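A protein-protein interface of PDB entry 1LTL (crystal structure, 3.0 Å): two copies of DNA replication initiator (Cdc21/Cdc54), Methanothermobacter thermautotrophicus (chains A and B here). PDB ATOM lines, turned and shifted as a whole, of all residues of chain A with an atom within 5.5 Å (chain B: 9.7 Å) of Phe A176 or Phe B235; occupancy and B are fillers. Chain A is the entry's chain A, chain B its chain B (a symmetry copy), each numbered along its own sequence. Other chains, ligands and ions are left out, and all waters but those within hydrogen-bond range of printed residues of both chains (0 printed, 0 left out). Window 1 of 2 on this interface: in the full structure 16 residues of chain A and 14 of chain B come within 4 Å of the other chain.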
ATOM      1  N   ARG A 127      -3.653 -26.796 -14.847  1.00  0.00           N
ATOM      2  CA  ARG A 127      -3.836 -25.371 -14.554  1.00  0.00           C
ATOM      3  C   ARG A 127      -3.727 -25.193 -13.059  1.00  0.00           C
ATOM      4  O   ARG A 127      -3.810 -26.149 -12.291  1.00  0.00           O
ATOM      5  CB  ARG A 127      -5.222 -24.846 -14.943  1.00  0.00           C
ATOM      6  CG  ARG A 127      -5.680 -25.088 -16.355  1.00  0.00           C
ATOM      7  CD  ARG A 127      -7.216 -24.925 -16.480  1.00  0.00           C
ATOM      8  NE  ARG A 127      -7.775 -25.652 -17.637  1.00  0.00           N
ATOM      9  CZ  ARG A 127      -7.628 -25.300 -18.919  1.00  0.00           C
ATOM     10  NH1 ARG A 127      -6.936 -24.202 -19.243  1.00  0.00           N
ATOM     11  NH2 ARG A 127      -8.157 -26.064 -19.877  1.00  0.00           N
ATOM     12  N   PRO A 128      -3.508 -23.964 -12.612  1.00  0.00           N
ATOM     13  CA  PRO A 128      -3.429 -23.850 -11.160  1.00  0.00           C
ATOM     14  C   PRO A 128      -4.814 -23.489 -10.576  1.00  0.00           C
ATOM     15  O   PRO A 128      -5.773 -23.200 -11.312  1.00  0.00           O
ATOM     16  CB  PRO A 128      -2.398 -22.743 -10.961  1.00  0.00           C
ATOM     17  CG  PRO A 128      -2.562 -21.903 -12.196  1.00  0.00           C
ATOM     18  CD  PRO A 128      -2.772 -22.885 -13.287  1.00  0.00           C
ATOM     19  N   ARG A 129      -4.924 -23.530  -9.252  1.00  0.00           N
ATOM     20  CA  ARG A 129      -6.161 -23.165  -8.593  1.00  0.00           C
ATOM     21  C   ARG A 129      -5.769 -22.668  -7.218  1.00  0.00           C
ATOM     22  O   ARG A 129      -4.756 -23.077  -6.678  1.00  0.00           O
ATOM     23  CB  ARG A 129      -7.105 -24.360  -8.471  1.00  0.00           C
ATOM     24  CG  ARG A 129      -7.022 -25.123  -7.156  1.00  0.00           C
ATOM     25  CD  ARG A 129      -8.242 -25.994  -7.005  1.00  0.00           C
ATOM     26  NE  ARG A 129      -8.074 -27.073  -6.027  1.00  0.00           N
ATOM     27  CZ  ARG A 129      -7.979 -26.905  -4.713  1.00  0.00           C
ATOM     28  NH1 ARG A 129      -8.026 -25.689  -4.180  1.00  0.00           N
ATOM     29  NH2 ARG A 129      -7.859 -27.966  -3.925  1.00  0.00           N
ATOM     30  N   ILE A 130      -6.567 -21.784  -6.643  1.00  0.00           N
ATOM     31  CA  ILE A 130      -6.226 -21.268  -5.340  1.00  0.00           C
ATOM     32  C   ILE A 130      -6.547 -22.292  -4.276  1.00  0.00           C
ATOM     33  O   ILE A 130      -7.655 -22.814  -4.247  1.00  0.00           O
ATOM     34  CB  ILE A 130      -6.996 -19.979  -5.049  1.00  0.00           C
ATOM     35  CG1 ILE A 130      -6.680 -18.956  -6.134  1.00  0.00           C
ATOM     36  CG2 ILE A 130      -6.646 -19.459  -3.678  1.00  0.00           C
ATOM     37  CD1 ILE A 130      -7.339 -17.639  -5.962  1.00  0.00           C
ATOM     38  N   VAL A 131      -5.583 -22.607  -3.415  1.00  0.00           N
ATOM     39  CA  VAL A 131      -5.838 -23.558  -2.332  1.00  0.00           C
ATOM     40  C   VAL A 131      -6.041 -22.784  -1.066  1.00  0.00           C
ATOM     41  O   VAL A 131      -6.828 -23.174  -0.227  1.00  0.00           O
ATOM     42  CB  VAL A 131      -4.666 -24.513  -2.065  1.00  0.00           C
ATOM     43  CG1 VAL A 131      -4.746 -25.716  -2.981  1.00  0.00           C
ATOM     44  CG2 VAL A 131      -3.358 -23.783  -2.243  1.00  0.00           C
ATOM     45  N   ASN A 151     -12.800 -24.991  -7.162  1.00  0.00           N
ATOM     46  CA  ASN A 151     -12.227 -23.903  -7.930  1.00  0.00           C
ATOM     47  C   ASN A 151     -13.141 -22.689  -7.767  1.00  0.00           C
ATOM     48  O   ASN A 151     -12.998 -21.689  -8.463  1.00  0.00           O
ATOM     49  CB  ASN A 151     -12.086 -24.267  -9.410  1.00  0.00           C
ATOM     50  CG  ASN A 151     -11.499 -23.121 -10.238  1.00  0.00           C
ATOM     51  OD1 ASN A 151     -10.375 -22.669  -9.994  1.00  0.00           O
ATOM     52  ND2 ASN A 151     -12.264 -22.646 -11.219  1.00  0.00           N
ATOM     53  N   GLN A 171      -5.785 -11.765  -4.646  1.00  0.00           N
ATOM     54  CA  GLN A 171      -5.073 -12.801  -5.388  1.00  0.00           C
ATOM     55  C   GLN A 171      -3.567 -12.852  -5.184  1.00  0.00           C
ATOM     56  O   GLN A 171      -3.008 -13.932  -5.012  1.00  0.00           O
ATOM     57  CB  GLN A 171      -5.347 -12.704  -6.883  1.00  0.00           C
ATOM     58  CG  GLN A 171      -4.684 -13.826  -7.660  1.00  0.00           C
ATOM     59  CD  GLN A 171      -4.966 -13.763  -9.155  1.00  0.00           C
ATOM     60  OE1 GLN A 171      -6.119 -13.644  -9.578  1.00  0.00           O
ATOM     61  NE2 GLN A 171      -3.911 -13.857  -9.964  1.00  0.00           N
ATOM     62  N   SER A 174      -2.566 -14.915  -2.276  1.00  0.00           N
ATOM     63  CA  SER A 174      -3.075 -16.258  -2.184  1.00  0.00           C
ATOM     64  C   SER A 174      -2.104 -17.310  -2.713  1.00  0.00           C
ATOM     65  O   SER A 174      -1.243 -17.010  -3.536  1.00  0.00           O
ATOM     66  CB  SER A 174      -4.408 -16.312  -2.914  1.00  0.00           C
ATOM     67  OG  SER A 174      -5.317 -15.432  -2.287  1.00  0.00           O
ATOM     68  N   GLU A 175      -2.239 -18.539  -2.220  1.00  0.00           N
ATOM     69  CA  GLU A 175      -1.376 -19.639  -2.641  1.00  0.00           C
ATOM     70  C   GLU A 175      -2.072 -20.518  -3.658  1.00  0.00           C
ATOM     71  O   GLU A 175      -3.231 -20.872  -3.492  1.00  0.00           O
ATOM     72  CB  GLU A 175      -0.960 -20.474  -1.426  1.00  0.00           C
ATOM     73  CG  GLU A 175       0.073 -19.802  -0.505  1.00  0.00           C
ATOM     74  CD  GLU A 175       0.243 -20.530   0.831  1.00  0.00           C
ATOM     75  OE1 GLU A 175       0.307 -21.790   0.844  1.00  0.00           O
ATOM     76  OE2 GLU A 175       0.325 -19.838   1.879  1.00  0.00           O
ATOM     77  N   PHE A 176      -1.357 -20.858  -4.718  1.00  0.00           N
ATOM     78  CA  PHE A 176      -1.913 -21.690  -5.763  1.00  0.00           C
ATOM     79  C   PHE A 176      -1.468 -23.132  -5.655  1.00  0.00           C
ATOM     80  O   PHE A 176      -0.695 -23.496  -4.777  1.00  0.00           O
ATOM     81  CB  PHE A 176      -1.546 -21.139  -7.136  1.00  0.00           C
ATOM     82  CG  PHE A 176      -2.247 -19.864  -7.470  1.00  0.00           C
ATOM     83  CD1 PHE A 176      -1.952 -18.692  -6.794  1.00  0.00           C
ATOM     84  CD2 PHE A 176      -3.252 -19.843  -8.428  1.00  0.00           C
ATOM     85  CE1 PHE A 176      -2.646 -17.519  -7.061  1.00  0.00           C
ATOM     86  CE2 PHE A 176      -3.956 -18.664  -8.701  1.00  0.00           C
ATOM     87  CZ  PHE A 176      -3.648 -17.505  -8.014  1.00  0.00           C
ATOM     88  N   LEU A 177      -1.934 -23.949  -6.582  1.00  0.00           N
ATOM     89  CA  LEU A 177      -1.622 -25.360  -6.539  1.00  0.00           C
ATOM     90  C   LEU A 177      -2.027 -26.011  -7.850  1.00  0.00           C
ATOM     91  O   LEU A 177      -3.081 -25.701  -8.391  1.00  0.00           O
ATOM     92  CB  LEU A 177      -2.368 -25.941  -5.357  1.00  0.00           C
ATOM     93  CG  LEU A 177      -2.613 -27.427  -5.258  1.00  0.00           C
ATOM     94  CD1 LEU A 177      -2.252 -27.868  -3.849  1.00  0.00           C
ATOM     95  CD2 LEU A 177      -4.070 -27.725  -5.586  1.00  0.00           C
ATOM     96  N   ASP A 178      -1.208 -26.903  -8.391  1.00  0.00           N
ATOM     97  CA  ASP A 178      -1.569 -27.489  -9.679  1.00  0.00           C
ATOM     98  C   ASP A 178      -2.698 -28.507  -9.620  1.00  0.00           C
ATOM     99  O   ASP A 178      -2.741 -29.368  -8.747  1.00  0.00           O
ATOM    100  CB  ASP A 178      -0.335 -28.089 -10.346  1.00  0.00           C
ATOM    101  CG  ASP A 178       0.701 -27.040 -10.692  1.00  0.00           C
ATOM    102  OD1 ASP A 178       0.371 -26.085 -11.455  1.00  0.00           O
ATOM    103  OD2 ASP A 178       1.851 -27.178 -10.197  1.00  0.00           O
ATOM    104  N   ARG B 106       4.710 -24.393 -13.787  1.00  0.00           N
ATOM    105  CA  ARG B 106       3.547 -24.671 -12.962  1.00  0.00           C
ATOM    106  C   ARG B 106       3.458 -23.716 -11.768  1.00  0.00           C
ATOM    107  O   ARG B 106       4.167 -22.714 -11.691  1.00  0.00           O
ATOM    108  CB  ARG B 106       3.605 -26.098 -12.426  1.00  0.00           C
ATOM    109  CG  ARG B 106       4.006 -27.180 -13.437  1.00  0.00           C
ATOM    110  CD  ARG B 106       2.827 -27.668 -14.250  1.00  0.00           C
ATOM    111  NE  ARG B 106       3.142 -28.757 -15.187  1.00  0.00           N
ATOM    112  CZ  ARG B 106       3.606 -29.951 -14.834  1.00  0.00           C
ATOM    113  NH1 ARG B 106       3.831 -30.235 -13.551  1.00  0.00           N
ATOM    114  NH2 ARG B 106       3.812 -30.876 -15.761  1.00  0.00           N
ATOM    115  N   SER B 107       2.612 -24.065 -10.806  1.00  0.00           N
ATOM    116  CA  SER B 107       2.373 -23.228  -9.641  1.00  0.00           C
ATOM    117  C   SER B 107       3.559 -22.772  -8.829  1.00  0.00           C
ATOM    118  O   SER B 107       3.576 -21.641  -8.342  1.00  0.00           O
ATOM    119  CB  SER B 107       1.393 -23.923  -8.707  1.00  0.00           C
ATOM    120  OG  SER B 107       0.308 -24.425  -9.449  1.00  0.00           O
ATOM    121  N   LYS B 108       4.546 -23.633  -8.644  1.00  0.00           N
ATOM    122  CA  LYS B 108       5.693 -23.237  -7.832  1.00  0.00           C
ATOM    123  C   LYS B 108       6.382 -21.980  -8.360  1.00  0.00           C
ATOM    124  O   LYS B 108       7.015 -21.248  -7.605  1.00  0.00           O
ATOM    125  CB  LYS B 108       6.706 -24.385  -7.757  1.00  0.00           C
ATOM    126  CG  LYS B 108       7.067 -24.964  -9.107  1.00  0.00           C
ATOM    127  CD  LYS B 108       8.401 -25.660  -9.066  1.00  0.00           C
ATOM    128  CE  LYS B 108       8.437 -26.757  -8.018  1.00  0.00           C
ATOM    129  NZ  LYS B 108       9.724 -27.501  -8.144  1.00  0.00           N
ATOM    130  N   PHE B 109       6.237 -21.738  -9.658  1.00  0.00           N
ATOM    131  CA  PHE B 109       6.851 -20.604 -10.313  1.00  0.00           C
ATOM    132  C   PHE B 109       5.946 -19.392 -10.457  1.00  0.00           C
ATOM    133  O   PHE B 109       6.243 -18.438 -11.175  1.00  0.00           O
ATOM    134  CB  PHE B 109       7.332 -21.045 -11.669  1.00  0.00           C
ATOM    135  CG  PHE B 109       8.406 -22.082 -11.607  1.00  0.00           C
ATOM    136  CD1 PHE B 109       8.367 -23.198 -12.441  1.00  0.00           C
ATOM    137  CD2 PHE B 109       9.505 -21.910 -10.764  1.00  0.00           C
ATOM    138  CE1 PHE B 109       9.414 -24.116 -12.441  1.00  0.00           C
ATOM    139  CE2 PHE B 109      10.544 -22.821 -10.763  1.00  0.00           C
ATOM    140  CZ  PHE B 109      10.498 -23.932 -11.609  1.00  0.00           C
ATOM    141  N   ILE B 110       4.820 -19.425  -9.779  1.00  0.00           N
ATOM    142  CA  ILE B 110       3.948 -18.302  -9.864  1.00  0.00           C
ATOM    143  C   ILE B 110       4.558 -17.230  -9.005  1.00  0.00           C
ATOM    144  O   ILE B 110       4.824 -17.437  -7.823  1.00  0.00           O
ATOM    145  CB  ILE B 110       2.537 -18.672  -9.413  1.00  0.00           C
ATOM    146  CG1 ILE B 110       1.847 -19.425 -10.558  1.00  0.00           C
ATOM    147  CG2 ILE B 110       1.768 -17.435  -9.015  1.00  0.00           C
ATOM    148  CD1 ILE B 110       0.387 -19.726 -10.345  1.00  0.00           C
ATOM    149  N   GLY B 111       4.821 -16.091  -9.641  1.00  0.00           N
ATOM    150  CA  GLY B 111       5.405 -14.949  -8.967  1.00  0.00           C
ATOM    151  C   GLY B 111       6.891 -15.091  -8.718  1.00  0.00           C
ATOM    152  O   GLY B 111       7.401 -14.544  -7.748  1.00  0.00           O
ATOM    153  N   MET B 152      -6.912  -4.859 -15.635  1.00  0.00           N
ATOM    154  CA  MET B 152      -8.133  -4.758 -14.863  1.00  0.00           C
ATOM    155  C   MET B 152      -7.915  -3.733 -13.781  1.00  0.00           C
ATOM    156  O   MET B 152      -7.054  -3.900 -12.928  1.00  0.00           O
ATOM    157  CB  MET B 152      -8.500  -6.088 -14.226  1.00  0.00           C
ATOM    158  CG  MET B 152      -9.256  -7.024 -15.149  1.00  0.00           C
ATOM    159  SD  MET B 152      -9.981  -8.427 -14.228  1.00  0.00           S
ATOM    160  CE  MET B 152      -8.579  -9.677 -14.222  1.00  0.00           C
ATOM    161  N   LEU B 224       6.501 -14.874 -13.658  1.00  0.00           N
ATOM    162  CA  LEU B 224       5.395 -15.713 -14.083  1.00  0.00           C
ATOM    163  C   LEU B 224       4.162 -15.273 -13.302  1.00  0.00           C
ATOM    164  O   LEU B 224       4.142 -15.267 -12.067  1.00  0.00           O
ATOM    165  CB  LEU B 224       5.705 -17.183 -13.839  1.00  0.00           C
ATOM    166  CG  LEU B 224       4.609 -18.158 -14.272  1.00  0.00           C
ATOM    167  CD1 LEU B 224       4.502 -18.324 -15.778  1.00  0.00           C
ATOM    168  CD2 LEU B 224       4.925 -19.480 -13.642  1.00  0.00           C
ATOM    169  N   ARG B 225       3.143 -14.862 -14.035  1.00  0.00           N
ATOM    170  CA  ARG B 225       1.916 -14.417 -13.405  1.00  0.00           C
ATOM    171  C   ARG B 225       0.805 -15.365 -13.848  1.00  0.00           C
ATOM    172  O   ARG B 225       0.987 -16.210 -14.731  1.00  0.00           O
ATOM    173  CB  ARG B 225       1.563 -12.991 -13.849  1.00  0.00           C
ATOM    174  CG  ARG B 225       2.631 -11.926 -13.720  1.00  0.00           C
ATOM    175  CD  ARG B 225       2.763 -11.332 -12.316  1.00  0.00           C
ATOM    176  NE  ARG B 225       3.369  -9.976 -12.323  1.00  0.00           N
ATOM    177  CZ  ARG B 225       2.987  -8.991 -13.143  1.00  0.00           C
ATOM    178  NH1 ARG B 225       2.013  -9.199 -14.026  1.00  0.00           N
ATOM    179  NH2 ARG B 225       3.555  -7.797 -13.079  1.00  0.00           N
ATOM    180  N   THR B 226      -0.357 -15.214 -13.233  1.00  0.00           N
ATOM    181  CA  THR B 226      -1.478 -16.046 -13.603  1.00  0.00           C
ATOM    182  C   THR B 226      -2.793 -15.272 -13.598  1.00  0.00           C
ATOM    183  O   THR B 226      -2.958 -14.319 -12.854  1.00  0.00           O
ATOM    184  CB  THR B 226      -1.611 -17.241 -12.655  1.00  0.00           C
ATOM    185  OG1 THR B 226      -2.440 -18.228 -13.278  1.00  0.00           O
ATOM    186  CG2 THR B 226      -2.239 -16.819 -11.332  1.00  0.00           C
ATOM    187  N   VAL B 227      -3.735 -15.687 -14.427  1.00  0.00           N
ATOM    188  CA  VAL B 227      -5.001 -14.999 -14.446  1.00  0.00           C
ATOM    189  C   VAL B 227      -6.144 -15.918 -14.786  1.00  0.00           C
ATOM    190  O   VAL B 227      -6.003 -16.748 -15.683  1.00  0.00           O
ATOM    191  CB  VAL B 227      -4.981 -13.822 -15.438  1.00  0.00           C
ATOM    192  CG1 VAL B 227      -4.708 -14.307 -16.831  1.00  0.00           C
ATOM    193  CG2 VAL B 227      -6.289 -13.089 -15.374  1.00  0.00           C
ATOM    194  N   ARG B 228      -7.268 -15.789 -14.064  1.00  0.00           N
ATOM    195  CA  ARG B 228      -8.454 -16.623 -14.341  1.00  0.00           C
ATOM    196  C   ARG B 228      -9.264 -15.974 -15.428  1.00  0.00           C
ATOM    197  O   ARG B 228      -9.615 -14.803 -15.355  1.00  0.00           O
ATOM    198  CB  ARG B 228      -9.364 -16.840 -13.106  1.00  0.00           C
ATOM    199  CG  ARG B 228      -9.785 -15.569 -12.383  1.00  0.00           C
ATOM    200  CD  ARG B 228     -10.977 -15.677 -11.356  1.00  0.00           C
ATOM    201  NE  ARG B 228     -10.864 -16.640 -10.237  1.00  0.00           N
ATOM    202  CZ  ARG B 228     -11.051 -17.958 -10.361  1.00  0.00           C
ATOM    203  NH1 ARG B 228     -11.340 -18.458 -11.558  1.00  0.00           N
ATOM    204  NH2 ARG B 228     -11.006 -18.763  -9.295  1.00  0.00           N
ATOM    205  N   ASP B 229      -9.541 -16.766 -16.447  1.00  0.00           N
ATOM    206  CA  ASP B 229     -10.306 -16.320 -17.584  1.00  0.00           C
ATOM    207  C   ASP B 229     -11.797 -16.303 -17.265  1.00  0.00           C
ATOM    208  O   ASP B 229     -12.297 -17.181 -16.563  1.00  0.00           O
ATOM    209  CB  ASP B 229     -10.001 -17.235 -18.770  1.00  0.00           C
ATOM    210  CG  ASP B 229     -11.136 -17.325 -19.739  1.00  0.00           C
ATOM    211  OD1 ASP B 229     -11.762 -16.282 -20.018  1.00  0.00           O
ATOM    212  OD2 ASP B 229     -11.397 -18.440 -20.238  1.00  0.00           O
ATOM    213  N   GLU B 230     -12.493 -15.280 -17.758  1.00  0.00           N
ATOM    214  CA  GLU B 230     -13.930 -15.168 -17.546  1.00  0.00           C
ATOM    215  C   GLU B 230     -14.611 -16.331 -18.227  1.00  0.00           C
ATOM    216  O   GLU B 230     -14.019 -16.972 -19.096  1.00  0.00           O
ATOM    217  CB  GLU B 230     -14.457 -13.863 -18.134  1.00  0.00           C
ATOM    218  CG  GLU B 230     -14.150 -12.679 -17.266  1.00  0.00           C
ATOM    219  CD  GLU B 230     -14.358 -13.010 -15.802  1.00  0.00           C
ATOM    220  OE1 GLU B 230     -15.330 -13.747 -15.493  1.00  0.00           O
ATOM    221  OE2 GLU B 230     -13.547 -12.538 -14.968  1.00  0.00           O
ATOM    222  N   ARG B 231     -15.860 -16.593 -17.857  1.00  0.00           N
ATOM    223  CA  ARG B 231     -16.596 -17.708 -18.455  1.00  0.00           C
ATOM    224  C   ARG B 231     -15.963 -18.983 -17.895  1.00  0.00           C
ATOM    225  O   ARG B 231     -16.431 -19.530 -16.889  1.00  0.00           O
ATOM    226  CB  ARG B 231     -16.475 -17.678 -19.994  1.00  0.00           C
ATOM    227  CG  ARG B 231     -16.840 -16.330 -20.635  1.00  0.00           C
ATOM    228  CD  ARG B 231     -17.042 -16.441 -22.149  1.00  0.00           C
ATOM    229  NE  ARG B 231     -17.305 -15.140 -22.776  1.00  0.00           N
ATOM    230  CZ  ARG B 231     -17.765 -14.978 -24.019  1.00  0.00           C
ATOM    231  NH1 ARG B 231     -18.021 -16.039 -24.779  1.00  0.00           N
ATOM    232  NH2 ARG B 231     -17.964 -13.755 -24.509  1.00  0.00           N
ATOM    233  N   THR B 232     -14.898 -19.438 -18.557  1.00  0.00           N
ATOM    234  CA  THR B 232     -14.135 -20.617 -18.150  1.00  0.00           C
ATOM    235  C   THR B 232     -13.380 -20.188 -16.920  1.00  0.00           C
ATOM    236  O   THR B 232     -12.241 -19.737 -17.025  1.00  0.00           O
ATOM    237  CB  THR B 232     -13.094 -20.984 -19.210  1.00  0.00           C
ATOM    238  OG1 THR B 232     -13.754 -21.414 -20.403  1.00  0.00           O
ATOM    239  CG2 THR B 232     -12.178 -22.076 -18.708  1.00  0.00           C
ATOM    240  N   LYS B 233     -14.001 -20.326 -15.758  1.00  0.00           N
ATOM    241  CA  LYS B 233     -13.385 -19.900 -14.499  1.00  0.00           C
ATOM    242  C   LYS B 233     -11.986 -20.451 -14.178  1.00  0.00           C
ATOM    243  O   LYS B 233     -11.545 -20.350 -13.048  1.00  0.00           O
ATOM    244  CB  LYS B 233     -14.334 -20.226 -13.344  1.00  0.00           C
ATOM    245  CG  LYS B 233     -15.710 -19.608 -13.484  1.00  0.00           C
ATOM    246  CD  LYS B 233     -15.681 -18.082 -13.348  1.00  0.00           C
ATOM    247  CE  LYS B 233     -16.494 -17.401 -14.456  1.00  0.00           C
ATOM    248  NZ  LYS B 233     -17.850 -18.027 -14.632  1.00  0.00           N
ATOM    249  N   ARG B 234     -11.300 -21.023 -15.163  1.00  0.00           N
ATOM    250  CA  ARG B 234      -9.959 -21.570 -14.953  1.00  0.00           C
ATOM    251  C   ARG B 234      -8.815 -20.561 -15.133  1.00  0.00           C
ATOM    252  O   ARG B 234      -8.903 -19.646 -15.950  1.00  0.00           O
ATOM    253  CB  ARG B 234      -9.707 -22.764 -15.887  1.00  0.00           C
ATOM    254  CG  ARG B 234     -10.284 -24.097 -15.401  1.00  0.00           C
ATOM    255  CD  ARG B 234     -11.632 -24.400 -16.038  1.00  0.00           C
ATOM    256  NE  ARG B 234     -11.524 -24.634 -17.484  1.00  0.00           N
ATOM    257  CZ  ARG B 234     -11.079 -25.759 -18.044  1.00  0.00           C
ATOM    258  NH1 ARG B 234     -10.692 -26.787 -17.283  1.00  0.00           N
ATOM    259  NH2 ARG B 234     -11.021 -25.850 -19.369  1.00  0.00           N
ATOM    260  N   PHE B 235      -7.746 -20.741 -14.356  1.00  0.00           N
ATOM    261  CA  PHE B 235      -6.578 -19.882 -14.436  1.00  0.00           C
ATOM    262  C   PHE B 235      -5.713 -20.279 -15.617  1.00  0.00           C
ATOM    263  O   PHE B 235      -5.891 -21.325 -16.222  1.00  0.00           O
ATOM    264  CB  PHE B 235      -5.742 -19.969 -13.171  1.00  0.00           C
ATOM    265  CG  PHE B 235      -6.237 -19.107 -12.058  1.00  0.00           C
ATOM    266  CD1 PHE B 235      -7.066 -19.615 -11.076  1.00  0.00           C
ATOM    267  CD2 PHE B 235      -5.851 -17.777 -11.967  1.00  0.00           C
ATOM    268  CE1 PHE B 235      -7.499 -18.808 -10.007  1.00  0.00           C
ATOM    269  CE2 PHE B 235      -6.286 -16.967 -10.894  1.00  0.00           C
ATOM    270  CZ  PHE B 235      -7.105 -17.489  -9.922  1.00  0.00           C
ATOM    271  N   LYS B 236      -4.762 -19.421 -15.939  1.00  0.00           N
ATOM    272  CA  LYS B 236      -3.868 -19.664 -17.051  1.00  0.00           C
ATOM    273  C   LYS B 236      -2.611 -18.894 -16.721  1.00  0.00           C
ATOM    274  O   LYS B 236      -2.694 -17.759 -16.267  1.00  0.00           O
ATOM    275  CB  LYS B 236      -4.494 -19.119 -18.328  1.00  0.00           C
ATOM    276  CG  LYS B 236      -3.766 -19.469 -19.609  1.00  0.00           C
ATOM    277  CD  LYS B 236      -3.744 -20.975 -19.857  1.00  0.00           C
ATOM    278  CE  LYS B 236      -3.941 -21.308 -21.345  1.00  0.00           C
ATOM    279  NZ  LYS B 236      -3.007 -20.600 -22.279  1.00  0.00           N
ATOM    280  N   ASN B 237      -1.448 -19.495 -16.928  1.00  0.00           N
ATOM    281  CA  ASN B 237      -0.225 -18.775 -16.620  1.00  0.00           C
ATOM    282  C   ASN B 237       0.344 -18.048 -17.806  1.00  0.00           C
ATOM    283  O   ASN B 237       0.174 -18.469 -18.946  1.00  0.00           O
ATOM    284  CB  ASN B 237       0.836 -19.713 -16.093  1.00  0.00           C
ATOM    285  CG  ASN B 237       0.455 -20.323 -14.790  1.00  0.00           C
ATOM    286  OD1 ASN B 237      -0.311 -19.745 -14.024  1.00  0.00           O
ATOM    287  ND2 ASN B 237       0.996 -21.497 -14.509  1.00  0.00           N
ATOM    288  N   PHE B 238       1.005 -16.934 -17.534  1.00  0.00           N
ATOM    289  CA  PHE B 238       1.660 -16.191 -18.586  1.00  0.00           C
ATOM    290  C   PHE B 238       2.924 -15.564 -18.022  1.00  0.00           C
ATOM    291  O   PHE B 238       3.130 -15.553 -16.802  1.00  0.00           O
ATOM    292  CB  PHE B 238       0.737 -15.128 -19.167  1.00  0.00           C
ATOM    293  CG  PHE B 238       0.474 -13.998 -18.249  1.00  0.00           C
ATOM    294  CD1 PHE B 238       1.232 -12.838 -18.323  1.00  0.00           C
ATOM    295  CD2 PHE B 238      -0.488 -14.109 -17.261  1.00  0.00           C
ATOM    296  CE1 PHE B 238       1.035 -11.810 -17.421  1.00  0.00           C
ATOM    297  CE2 PHE B 238      -0.686 -13.088 -16.362  1.00  0.00           C
ATOM    298  CZ  PHE B 238       0.078 -11.932 -16.439  1.00  0.00           C
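Among the printed residues, merely in contact across the chains: Asp A178 with Arg B106, Leu A177 with Ser B107, Pro A128 with Ser B107, Phe A176 with Phe B235, Gln A171 with Phe B235, Pro A128 with Asn B237, Asn A151 with Arg B228, Phe A176 with Thr B226, Pro A128 with Phe B235, Arg A127 with Phe B235, Pro A128 with Thr B226, Phe A176 with Ile B110 and Ile A130 with Phe B235.
Of the 12 printed residues of chain A, 8 touch a printed residue of chain B. Printed residues of chain A that touch a printed residue of chain B: Arg A127, Pro A128, Ile A130, Asn A151, Gln A171, Phe A176, Leu A177 and Asp A178. Hydrophobic or aromatic side chains of chain A that line the printed part of chain B: Pro A128, Ile A130 and Phe A176. Printed residues of chain B that touch a printed residue of chain A: Arg B106, Ser B107, Ile B110, Thr B226, Arg B228, Lys B233, Arg B234, Phe B235 and Asn B237. Hydrophobic or aromatic side chains of chain B within 4 Å of the printed part of chain A: Ile B110 and Phe B235. Among the printed residues, 17 pairs touch across the chains.
O of Thr B226 is in hydrogen-bond range of NE2 of Gln A171 (3.1 Å). The guanidinium group of Arg A127 sits close to the guanidinium group of Arg B234, at 2.9 Å. O of Lys B233 lies within hydrogen-bond range of ND2 of Asn A151. The side-chain hydroxyl of Ser B107 lies within hydrogen-bond range of the side-chain carboxylate of Asp A178.
The side-chain amide oxygen of Asn B237 sits at hydrogen-bond distance from the side-chain hydroxyl of Thr B226, at 2.7 Å. The backbone carbonyl oxygen (O) of Arg A129 sits at hydrogen-bond distance from the backbone NH (N) of Leu A177 (3.0 Å). N of Asp B229 lies within hydrogen-bond range of O of Arg B234 (3.0 Å). The backbone carbonyl oxygen of Lys B233 sits at hydrogen-bond distance from the guanidinium group of Arg B228, 2.4 Å away. NZ of Lys B233 sits at hydrogen-bond distance from O of Arg B231. The backbone carbonyl oxygen (O) of Lys B236 lies within hydrogen-bond range of the side-chain hydroxyl (OG1) of Thr B226, at 3.0 Å.
No position is printed for both chains.
Printed residues of chain B within 4 Å of Gln A171: Thr B226 and Phe B235. Phe A176 touches just these residues of chain B: Ile B110, Thr B226 and Phe B235. Of chain B, only Ser B107 (3.2 Å) comes within 4 Å of Leu A177. Of the printed residues of chain A, Ile B110 touches Phe A176. Leu B224 touches none of the printed residues of chain A. Printed residues of chain A within 4 Å of Arg B228: Asn A151 (3.6 Å). Asp B229 touches none of the printed residues of chain A. Printed residues of chain A within 4 Å of Lys B233: Asn A151. Of the printed residues of chain A, Arg B234 touches Arg A127. Phe B235 touches five residues of chain A. The nearest residue of chain B that does not touch Phe A176 is Ser B107 (4.3 Å). The nearest residue of chain A that does not touch Phe B235 is Arg A129 (4.4 Å).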
